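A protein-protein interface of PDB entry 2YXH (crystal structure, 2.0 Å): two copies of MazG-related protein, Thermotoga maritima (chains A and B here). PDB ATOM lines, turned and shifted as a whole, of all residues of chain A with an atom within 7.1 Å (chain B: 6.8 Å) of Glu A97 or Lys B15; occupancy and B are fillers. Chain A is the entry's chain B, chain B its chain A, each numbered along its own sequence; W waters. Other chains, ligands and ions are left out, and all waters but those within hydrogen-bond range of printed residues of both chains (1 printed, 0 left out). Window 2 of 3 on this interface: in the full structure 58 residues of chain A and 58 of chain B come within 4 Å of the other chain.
NH1 of Arg B11 is in hydrogen-bond range of O of Leu A94, at 3.0 Å. The side-chain amino group of Lys B15 lies within hydrogen-bond range of the backbone carbonyl oxygen of Trp A96 (2.9 Å). The side-chain amino group of Lys B15 is in hydrogen-bond range of the backbone carbonyl oxygen of Glu A97, at 3.1 Å. The side-chain sulfur of Cys B16 is in hydrogen-bond range of the indole nitrogen of Trp A93, at 3.5 Å.
O of Pro A92 lies close to NE1 of Trp A96 (3.5 Å). The side-chain sulfur (SG) of Cys B16 lies close to the backbone NH (N) of Trp B18 (3.6 Å).
Among the printed residues, merely in contact across the chains: Leu A94 with Lys B15, Ile A100 with Pro B17, Phe A95 with Arg B11, Leu A94 with Ser B12, Trp A93 with Pro B17, Trp A93 with Lys B15 and Leu A94 with Cys B16.
Of the printed residues of chain B, Trp A93 touches Lys B15 (3.9 Å), Cys B16 (3.5 Å) and Pro B17 (3.9 Å). Of the printed residues of chain B, Leu A94 touches Arg B11, Ser B12, Lys B15 and Cys B16. Of the printed residues of chain B, Phe A95 touches Arg B11. Of the printed residues of chain B, Glu A97 touches Lys B15. Of the printed residues of chain A, Arg B11 touches Leu A94 (3.0 Å) and Phe A95 (3.5 Å). Lys B15 touches four residues of chain A. Of the printed residues of chain A, Cys B16 touches Trp A93 (3.5 Å) and Leu A94 (3.9 Å). The nearest printed residue of chain B that does not touch Glu A97 is Arg B14 (6.8 Å). The nearest residue of chain A that does not touch Lys B15 is Lys A99 (4.7 Å).
Printed residues of chain A that touch a printed residue of chain B: Trp A93, Leu A94, Phe A95, Trp A96, Glu A97 and Ile A100. Along chain A the printed residues that touch a printed residue of chain B span positions 93 to 100. Of the 10 printed residues of chain B, 5 touch a printed residue of chain A. Hydrophobic or aromatic side chains of chain B that line the printed part of chain A: Pro B17. Along chain B the printed residues that touch a printed residue of chain A span positions 11 to 17. Among the printed residues, 11 pairs touch across the chains. Among the printed residues, no Asp or Glu carboxylate lies within 4 Å of a Lys or Arg side-chain nitrogen of the other chain.
No position is printed for both chains. Of the 11 pairs that touch across the chains among the printed residues, none has its exchanged pair printed and touching as well.
Water W1 bridges the backbone NH (N) of Ile A100 (2.8 Å) and the backbone carbonyl oxygen (O) of Lys B15 (2.8 Å).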
ATOM      1  N   PRO A  92     -23.278 -32.707  11.233  1.00  0.00           N
ATOM      2  CA  PRO A  92     -22.272 -33.360  10.393  1.00  0.00           C
ATOM      3  C   PRO A  92     -20.948 -32.632  10.437  1.00  0.00           C
ATOM      4  O   PRO A  92     -19.913 -33.227  10.102  1.00  0.00           O
ATOM      5  CB  PRO A  92     -22.843 -33.266   8.964  1.00  0.00           C
ATOM      6  CG  PRO A  92     -23.957 -32.145   9.041  1.00  0.00           C
ATOM      7  CD  PRO A  92     -24.468 -32.207  10.483  1.00  0.00           C
ATOM      8  N   TRP A  93     -20.980 -31.349  10.741  1.00  0.00           N
ATOM      9  CA  TRP A  93     -19.750 -30.559  10.813  1.00  0.00           C
ATOM     10  C   TRP A  93     -18.696 -31.068  11.828  1.00  0.00           C
ATOM     11  O   TRP A  93     -17.506 -30.719  11.729  1.00  0.00           O
ATOM     12  CB  TRP A  93     -20.040 -29.082  11.077  1.00  0.00           C
ATOM     13  CG  TRP A  93     -20.796 -28.793  12.337  1.00  0.00           C
ATOM     14  CD1 TRP A  93     -20.272 -28.583  13.595  1.00  0.00           C
ATOM     15  CD2 TRP A  93     -22.237 -28.677  12.463  1.00  0.00           C
ATOM     16  NE1 TRP A  93     -21.308 -28.345  14.524  1.00  0.00           N
ATOM     17  CE2 TRP A  93     -22.523 -28.395  13.854  1.00  0.00           C
ATOM     18  CE3 TRP A  93     -23.311 -28.787  11.559  1.00  0.00           C
ATOM     19  CZ2 TRP A  93     -23.862 -28.146  14.327  1.00  0.00           C
ATOM     20  CZ3 TRP A  93     -24.676 -28.567  12.052  1.00  0.00           C
ATOM     21  CH2 TRP A  93     -24.912 -28.287  13.424  1.00  0.00           C
ATOM     22  N   LEU A  94     -19.095 -31.964  12.727  1.00  0.00           N
ATOM     23  CA  LEU A  94     -18.166 -32.487  13.677  1.00  0.00           C
ATOM     24  C   LEU A  94     -17.137 -33.434  13.019  1.00  0.00           C
ATOM     25  O   LEU A  94     -16.106 -33.716  13.646  1.00  0.00           O
ATOM     26  CB  LEU A  94     -18.911 -33.271  14.736  1.00  0.00           C
ATOM     27  CG  LEU A  94     -20.026 -32.546  15.526  1.00  0.00           C
ATOM     28  CD1 LEU A  94     -20.627 -33.499  16.620  1.00  0.00           C
ATOM     29  CD2 LEU A  94     -19.391 -31.327  16.256  1.00  0.00           C
ATOM     30  N   PHE A  95     -17.464 -33.932  11.828  1.00  0.00           N
ATOM     31  CA  PHE A  95     -16.578 -34.817  11.071  1.00  0.00           C
ATOM     32  C   PHE A  95     -16.094 -34.161   9.815  1.00  0.00           C
ATOM     33  O   PHE A  95     -15.653 -34.852   8.917  1.00  0.00           O
ATOM     34  CB  PHE A  95     -17.314 -36.081  10.701  1.00  0.00           C
ATOM     35  CG  PHE A  95     -17.849 -36.790  11.906  1.00  0.00           C
ATOM     36  CD1 PHE A  95     -17.013 -37.662  12.646  1.00  0.00           C
ATOM     37  CD2 PHE A  95     -19.159 -36.496  12.377  1.00  0.00           C
ATOM     38  CE1 PHE A  95     -17.477 -38.273  13.801  1.00  0.00           C
ATOM     39  CE2 PHE A  95     -19.630 -37.067  13.494  1.00  0.00           C
ATOM     40  CZ  PHE A  95     -18.807 -37.964  14.221  1.00  0.00           C
ATOM     41  N   TRP A  96     -16.177 -32.833   9.741  1.00  0.00           N
ATOM     42  CA  TRP A  96     -15.631 -32.110   8.590  1.00  0.00           C
ATOM     43  C   TRP A  96     -14.385 -31.435   9.029  1.00  0.00           C
ATOM     44  O   TRP A  96     -14.339 -30.917  10.147  1.00  0.00           O
ATOM     45  CB  TRP A  96     -16.588 -31.056   8.120  1.00  0.00           C
ATOM     46  CG  TRP A  96     -17.838 -31.606   7.545  1.00  0.00           C
ATOM     47  CD1 TRP A  96     -18.112 -32.881   7.216  1.00  0.00           C
ATOM     48  CD2 TRP A  96     -18.952 -30.845   7.179  1.00  0.00           C
ATOM     49  NE1 TRP A  96     -19.371 -32.980   6.660  1.00  0.00           N
ATOM     50  CE2 TRP A  96     -19.917 -31.725   6.670  1.00  0.00           C
ATOM     51  CE3 TRP A  96     -19.277 -29.477   7.311  1.00  0.00           C
ATOM     52  CZ2 TRP A  96     -21.194 -31.283   6.278  1.00  0.00           C
ATOM     53  CZ3 TRP A  96     -20.483 -29.067   6.896  1.00  0.00           C
ATOM     54  CH2 TRP A  96     -21.439 -29.959   6.365  1.00  0.00           C
ATOM     55  N   GLU A  97     -13.364 -31.400   8.158  1.00  0.00           N
ATOM     56  CA  GLU A  97     -12.103 -30.688   8.566  1.00  0.00           C
ATOM     57  C   GLU A  97     -12.205 -29.223   8.958  1.00  0.00           C
ATOM     58  O   GLU A  97     -11.747 -28.817  10.031  1.00  0.00           O
ATOM     59  CB  GLU A  97     -11.011 -30.814   7.534  1.00  0.00           C
ATOM     60  CG  GLU A  97      -9.650 -30.417   8.116  1.00  0.00           C
ATOM     61  CD  GLU A  97      -8.521 -30.652   7.152  1.00  0.00           C
ATOM     62  OE1 GLU A  97      -8.748 -30.484   5.937  1.00  0.00           O
ATOM     63  OE2 GLU A  97      -7.426 -31.016   7.610  1.00  0.00           O
ATOM     64  N   GLU A  98     -12.790 -28.426   8.083  1.00  0.00           N
ATOM     65  CA  GLU A  98     -12.719 -27.019   8.259  1.00  0.00           C
ATOM     66  C   GLU A  98     -13.871 -26.618   9.132  1.00  0.00           C
ATOM     67  O   GLU A  98     -14.918 -27.260   9.091  1.00  0.00           O
ATOM     68  CB  GLU A  98     -12.801 -26.315   6.895  1.00  0.00           C
ATOM     69  CG  GLU A  98     -11.731 -26.750   5.831  1.00  0.00           C
ATOM     70  CD  GLU A  98     -10.261 -26.527   6.288  1.00  0.00           C
ATOM     71  OE1 GLU A  98      -9.920 -25.426   6.820  1.00  0.00           O
ATOM     72  OE2 GLU A  98      -9.446 -27.475   6.112  1.00  0.00           O
ATOM     73  N   LYS A  99     -13.683 -25.567   9.926  1.00  0.00           N
ATOM     74  CA  LYS A  99     -14.736 -25.121  10.845  1.00  0.00           C
ATOM     75  C   LYS A  99     -15.793 -24.378  10.054  1.00  0.00           C
ATOM     76  O   LYS A  99     -15.553 -23.978   8.881  1.00  0.00           O
ATOM     77  CB  LYS A  99     -14.206 -24.236  11.973  1.00  0.00           C
ATOM     78  CG  LYS A  99     -12.933 -24.839  12.627  1.00  0.00           C
ATOM     79  CD  LYS A  99     -12.021 -23.733  13.294  1.00  0.00           C
ATOM     80  CE  LYS A  99     -10.485 -24.134  13.331  1.00  0.00           C
ATOM     81  NZ  LYS A  99      -9.600 -23.203  14.165  1.00  0.00           N
ATOM     82  N   ILE A 100     -16.960 -24.191  10.695  1.00  0.00           N
ATOM     83  CA  ILE A 100     -18.069 -23.535  10.038  1.00  0.00           C
ATOM     84  C   ILE A 100     -18.676 -22.601  11.015  1.00  0.00           C
ATOM     85  O   ILE A 100     -18.509 -22.750  12.231  1.00  0.00           O
ATOM     86  CB  ILE A 100     -19.153 -24.528   9.465  1.00  0.00           C
ATOM     87  CG1 ILE A 100     -20.122 -25.086  10.539  1.00  0.00           C
ATOM     88  CG2 ILE A 100     -18.498 -25.698   8.635  1.00  0.00           C
ATOM     89  CD1 ILE A 100     -21.430 -25.781   9.839  1.00  0.00           C
ATOM     90  N   GLU B  10     -15.419 -34.851  22.277  1.00  0.00           N
ATOM     91  CA  GLU B  10     -14.129 -34.124  21.985  1.00  0.00           C
ATOM     92  C   GLU B  10     -14.225 -33.270  20.710  1.00  0.00           C
ATOM     93  O   GLU B  10     -13.740 -32.089  20.667  1.00  0.00           O
ATOM     94  CB  GLU B  10     -12.849 -34.981  21.959  1.00  0.00           C
ATOM     95  CG  GLU B  10     -11.597 -34.100  21.460  1.00  0.00           C
ATOM     96  CD  GLU B  10     -11.001 -33.000  22.489  1.00  0.00           C
ATOM     97  OE1 GLU B  10     -11.255 -33.130  23.733  1.00  0.00           O
ATOM     98  OE2 GLU B  10     -10.263 -32.028  22.054  1.00  0.00           O
ATOM     99  N   ARG B  11     -14.878 -33.833  19.683  1.00  0.00           N
ATOM    100  CA  ARG B  11     -14.965 -33.155  18.392  1.00  0.00           C
ATOM    101  C   ARG B  11     -15.795 -31.886  18.571  1.00  0.00           C
ATOM    102  O   ARG B  11     -15.530 -30.900  17.936  1.00  0.00           O
ATOM    103  CB  ARG B  11     -15.644 -34.045  17.355  1.00  0.00           C
ATOM    104  CG  ARG B  11     -14.704 -35.099  16.792  1.00  0.00           C
ATOM    105  CD  ARG B  11     -15.491 -36.056  15.928  1.00  0.00           C
ATOM    106  NE  ARG B  11     -14.575 -37.037  15.395  1.00  0.00           N
ATOM    107  CZ  ARG B  11     -13.720 -36.762  14.419  1.00  0.00           C
ATOM    108  NH1 ARG B  11     -13.726 -35.562  13.837  1.00  0.00           N
ATOM    109  NH2 ARG B  11     -12.863 -37.705  14.032  1.00  0.00           N
ATOM    110  N   SER B  12     -16.778 -31.938  19.431  1.00  0.00           N
ATOM    111  CA  SER B  12     -17.613 -30.718  19.681  1.00  0.00           C
ATOM    112  C   SER B  12     -16.874 -29.577  20.404  1.00  0.00           C
ATOM    113  O   SER B  12     -17.165 -28.388  20.197  1.00  0.00           O
ATOM    114  CB  SER B  12     -18.754 -31.128  20.580  1.00  0.00           C
ATOM    115  OG  SER B  12     -19.670 -32.030  19.951  1.00  0.00           O
ATOM    116  N   LEU B  13     -15.993 -29.940  21.330  1.00  0.00           N
ATOM    117  CA  LEU B  13     -15.188 -28.945  22.026  1.00  0.00           C
ATOM    118  C   LEU B  13     -14.335 -28.258  20.985  1.00  0.00           C
ATOM    119  O   LEU B  13     -14.214 -27.027  20.994  1.00  0.00           O
ATOM    120  CB  LEU B  13     -14.308 -29.605  23.098  1.00  0.00           C
ATOM    121  CG  LEU B  13     -15.148 -29.900  24.347  1.00  0.00           C
ATOM    122  CD1 LEU B  13     -14.391 -30.832  25.332  1.00  0.00           C
ATOM    123  CD2 LEU B  13     -15.760 -28.607  24.972  1.00  0.00           C
ATOM    124  N   ARG B  14     -13.797 -29.065  20.059  1.00  0.00           N
ATOM    125  CA  ARG B  14     -12.867 -28.566  19.108  1.00  0.00           C
ATOM    126  C   ARG B  14     -13.436 -27.832  17.940  1.00  0.00           C
ATOM    127  O   ARG B  14     -12.709 -27.037  17.326  1.00  0.00           O
ATOM    128  CB  ARG B  14     -11.979 -29.657  18.609  1.00  0.00           C
ATOM    129  CG  ARG B  14     -10.728 -29.790  19.478  1.00  0.00           C
ATOM    130  CD  ARG B  14      -9.722 -30.789  18.828  1.00  0.00           C
ATOM    131  NE  ARG B  14     -10.309 -32.060  18.315  1.00  0.00           N
ATOM    132  CZ  ARG B  14     -10.458 -32.413  17.017  1.00  0.00           C
ATOM    133  NH1 ARG B  14     -10.096 -31.576  15.996  1.00  0.00           N
ATOM    134  NH2 ARG B  14     -10.993 -33.630  16.743  1.00  0.00           N
ATOM    135  N   LYS B  15     -14.716 -28.049  17.622  1.00  0.00           N
ATOM    136  CA  LYS B  15     -15.174 -27.648  16.302  1.00  0.00           C
ATOM    137  C   LYS B  15     -16.494 -26.946  16.300  1.00  0.00           C
ATOM    138  O   LYS B  15     -16.779 -26.161  15.416  1.00  0.00           O
ATOM    139  CB  LYS B  15     -15.328 -28.840  15.384  1.00  0.00           C
ATOM    140  CG  LYS B  15     -14.074 -29.729  15.220  1.00  0.00           C
ATOM    141  CD  LYS B  15     -14.538 -30.829  14.286  1.00  0.00           C
ATOM    142  CE  LYS B  15     -13.439 -31.389  13.389  1.00  0.00           C
ATOM    143  NZ  LYS B  15     -12.856 -30.332  12.530  1.00  0.00           N
ATOM    144  N   CYS B  16     -17.338 -27.301  17.234  1.00  0.00           N
ATOM    145  CA  CYS B  16     -18.720 -26.806  17.254  1.00  0.00           C
ATOM    146  C   CYS B  16     -19.017 -25.360  17.710  1.00  0.00           C
ATOM    147  O   CYS B  16     -18.878 -24.999  18.894  1.00  0.00           O
ATOM    148  CB  CYS B  16     -19.575 -27.804  18.022  1.00  0.00           C
ATOM    149  SG  CYS B  16     -21.261 -27.350  17.842  1.00  0.00           S
ATOM    150  N   PRO B  17     -19.516 -24.531  16.777  1.00  0.00           N
ATOM    151  CA  PRO B  17     -19.782 -23.104  17.102  1.00  0.00           C
ATOM    152  C   PRO B  17     -21.044 -22.873  17.999  1.00  0.00           C
ATOM    153  O   PRO B  17     -21.152 -21.879  18.690  1.00  0.00           O
ATOM    154  CB  PRO B  17     -19.929 -22.464  15.698  1.00  0.00           C
ATOM    155  CG  PRO B  17     -20.555 -23.590  14.864  1.00  0.00           C
ATOM    156  CD  PRO B  17     -19.765 -24.838  15.346  1.00  0.00           C
ATOM    157  N   TRP B  18     -21.986 -23.813  17.989  1.00  0.00           N
ATOM    158  CA  TRP B  18     -23.106 -23.787  18.872  1.00  0.00           C
ATOM    159  C   TRP B  18     -22.589 -24.086  20.303  1.00  0.00           C
ATOM    160  O   TRP B  18     -22.967 -23.366  21.280  1.00  0.00           O
ATOM    161  CB  TRP B  18     -24.200 -24.788  18.406  1.00  0.00           C
ATOM    162  CG  TRP B  18     -25.251 -24.937  19.374  1.00  0.00           C
ATOM    163  CD1 TRP B  18     -26.377 -24.099  19.527  1.00  0.00           C
ATOM    164  CD2 TRP B  18     -25.322 -25.899  20.424  1.00  0.00           C
ATOM    165  NE1 TRP B  18     -27.130 -24.545  20.584  1.00  0.00           N
ATOM    166  CE2 TRP B  18     -26.506 -25.637  21.159  1.00  0.00           C
ATOM    167  CE3 TRP B  18     -24.522 -26.994  20.804  1.00  0.00           C
ATOM    168  CZ2 TRP B  18     -26.904 -26.439  22.237  1.00  0.00           C
ATOM    169  CZ3 TRP B  18     -24.907 -27.762  21.859  1.00  0.00           C
ATOM    170  CH2 TRP B  18     -26.087 -27.466  22.591  1.00  0.00           C
ATOM    171  N   GLU B  20     -19.683 -23.768  21.689  1.00  0.00           N
ATOM    172  CA  GLU B  20     -18.822 -22.618  22.138  1.00  0.00           C
ATOM    173  C   GLU B  20     -19.671 -21.546  22.856  1.00  0.00           C
ATOM    174  O   GLU B  20     -19.206 -20.929  23.879  1.00  0.00           O
ATOM    175  CB  GLU B  20     -18.097 -22.004  20.943  1.00  0.00           C
ATOM    176  CG  GLU B  20     -17.609 -20.622  21.173  1.00  0.00           C
ATOM    177  CD  GLU B  20     -16.512 -20.198  20.162  1.00  0.00           C
ATOM    178  OE1 GLU B  20     -16.368 -20.881  19.108  1.00  0.00           O
ATOM    179  OE2 GLU B  20     -15.811 -19.158  20.423  1.00  0.00           O
HETATM  180  O   HOH W   1     -17.578 -26.072  12.688  1.00  0.00           O
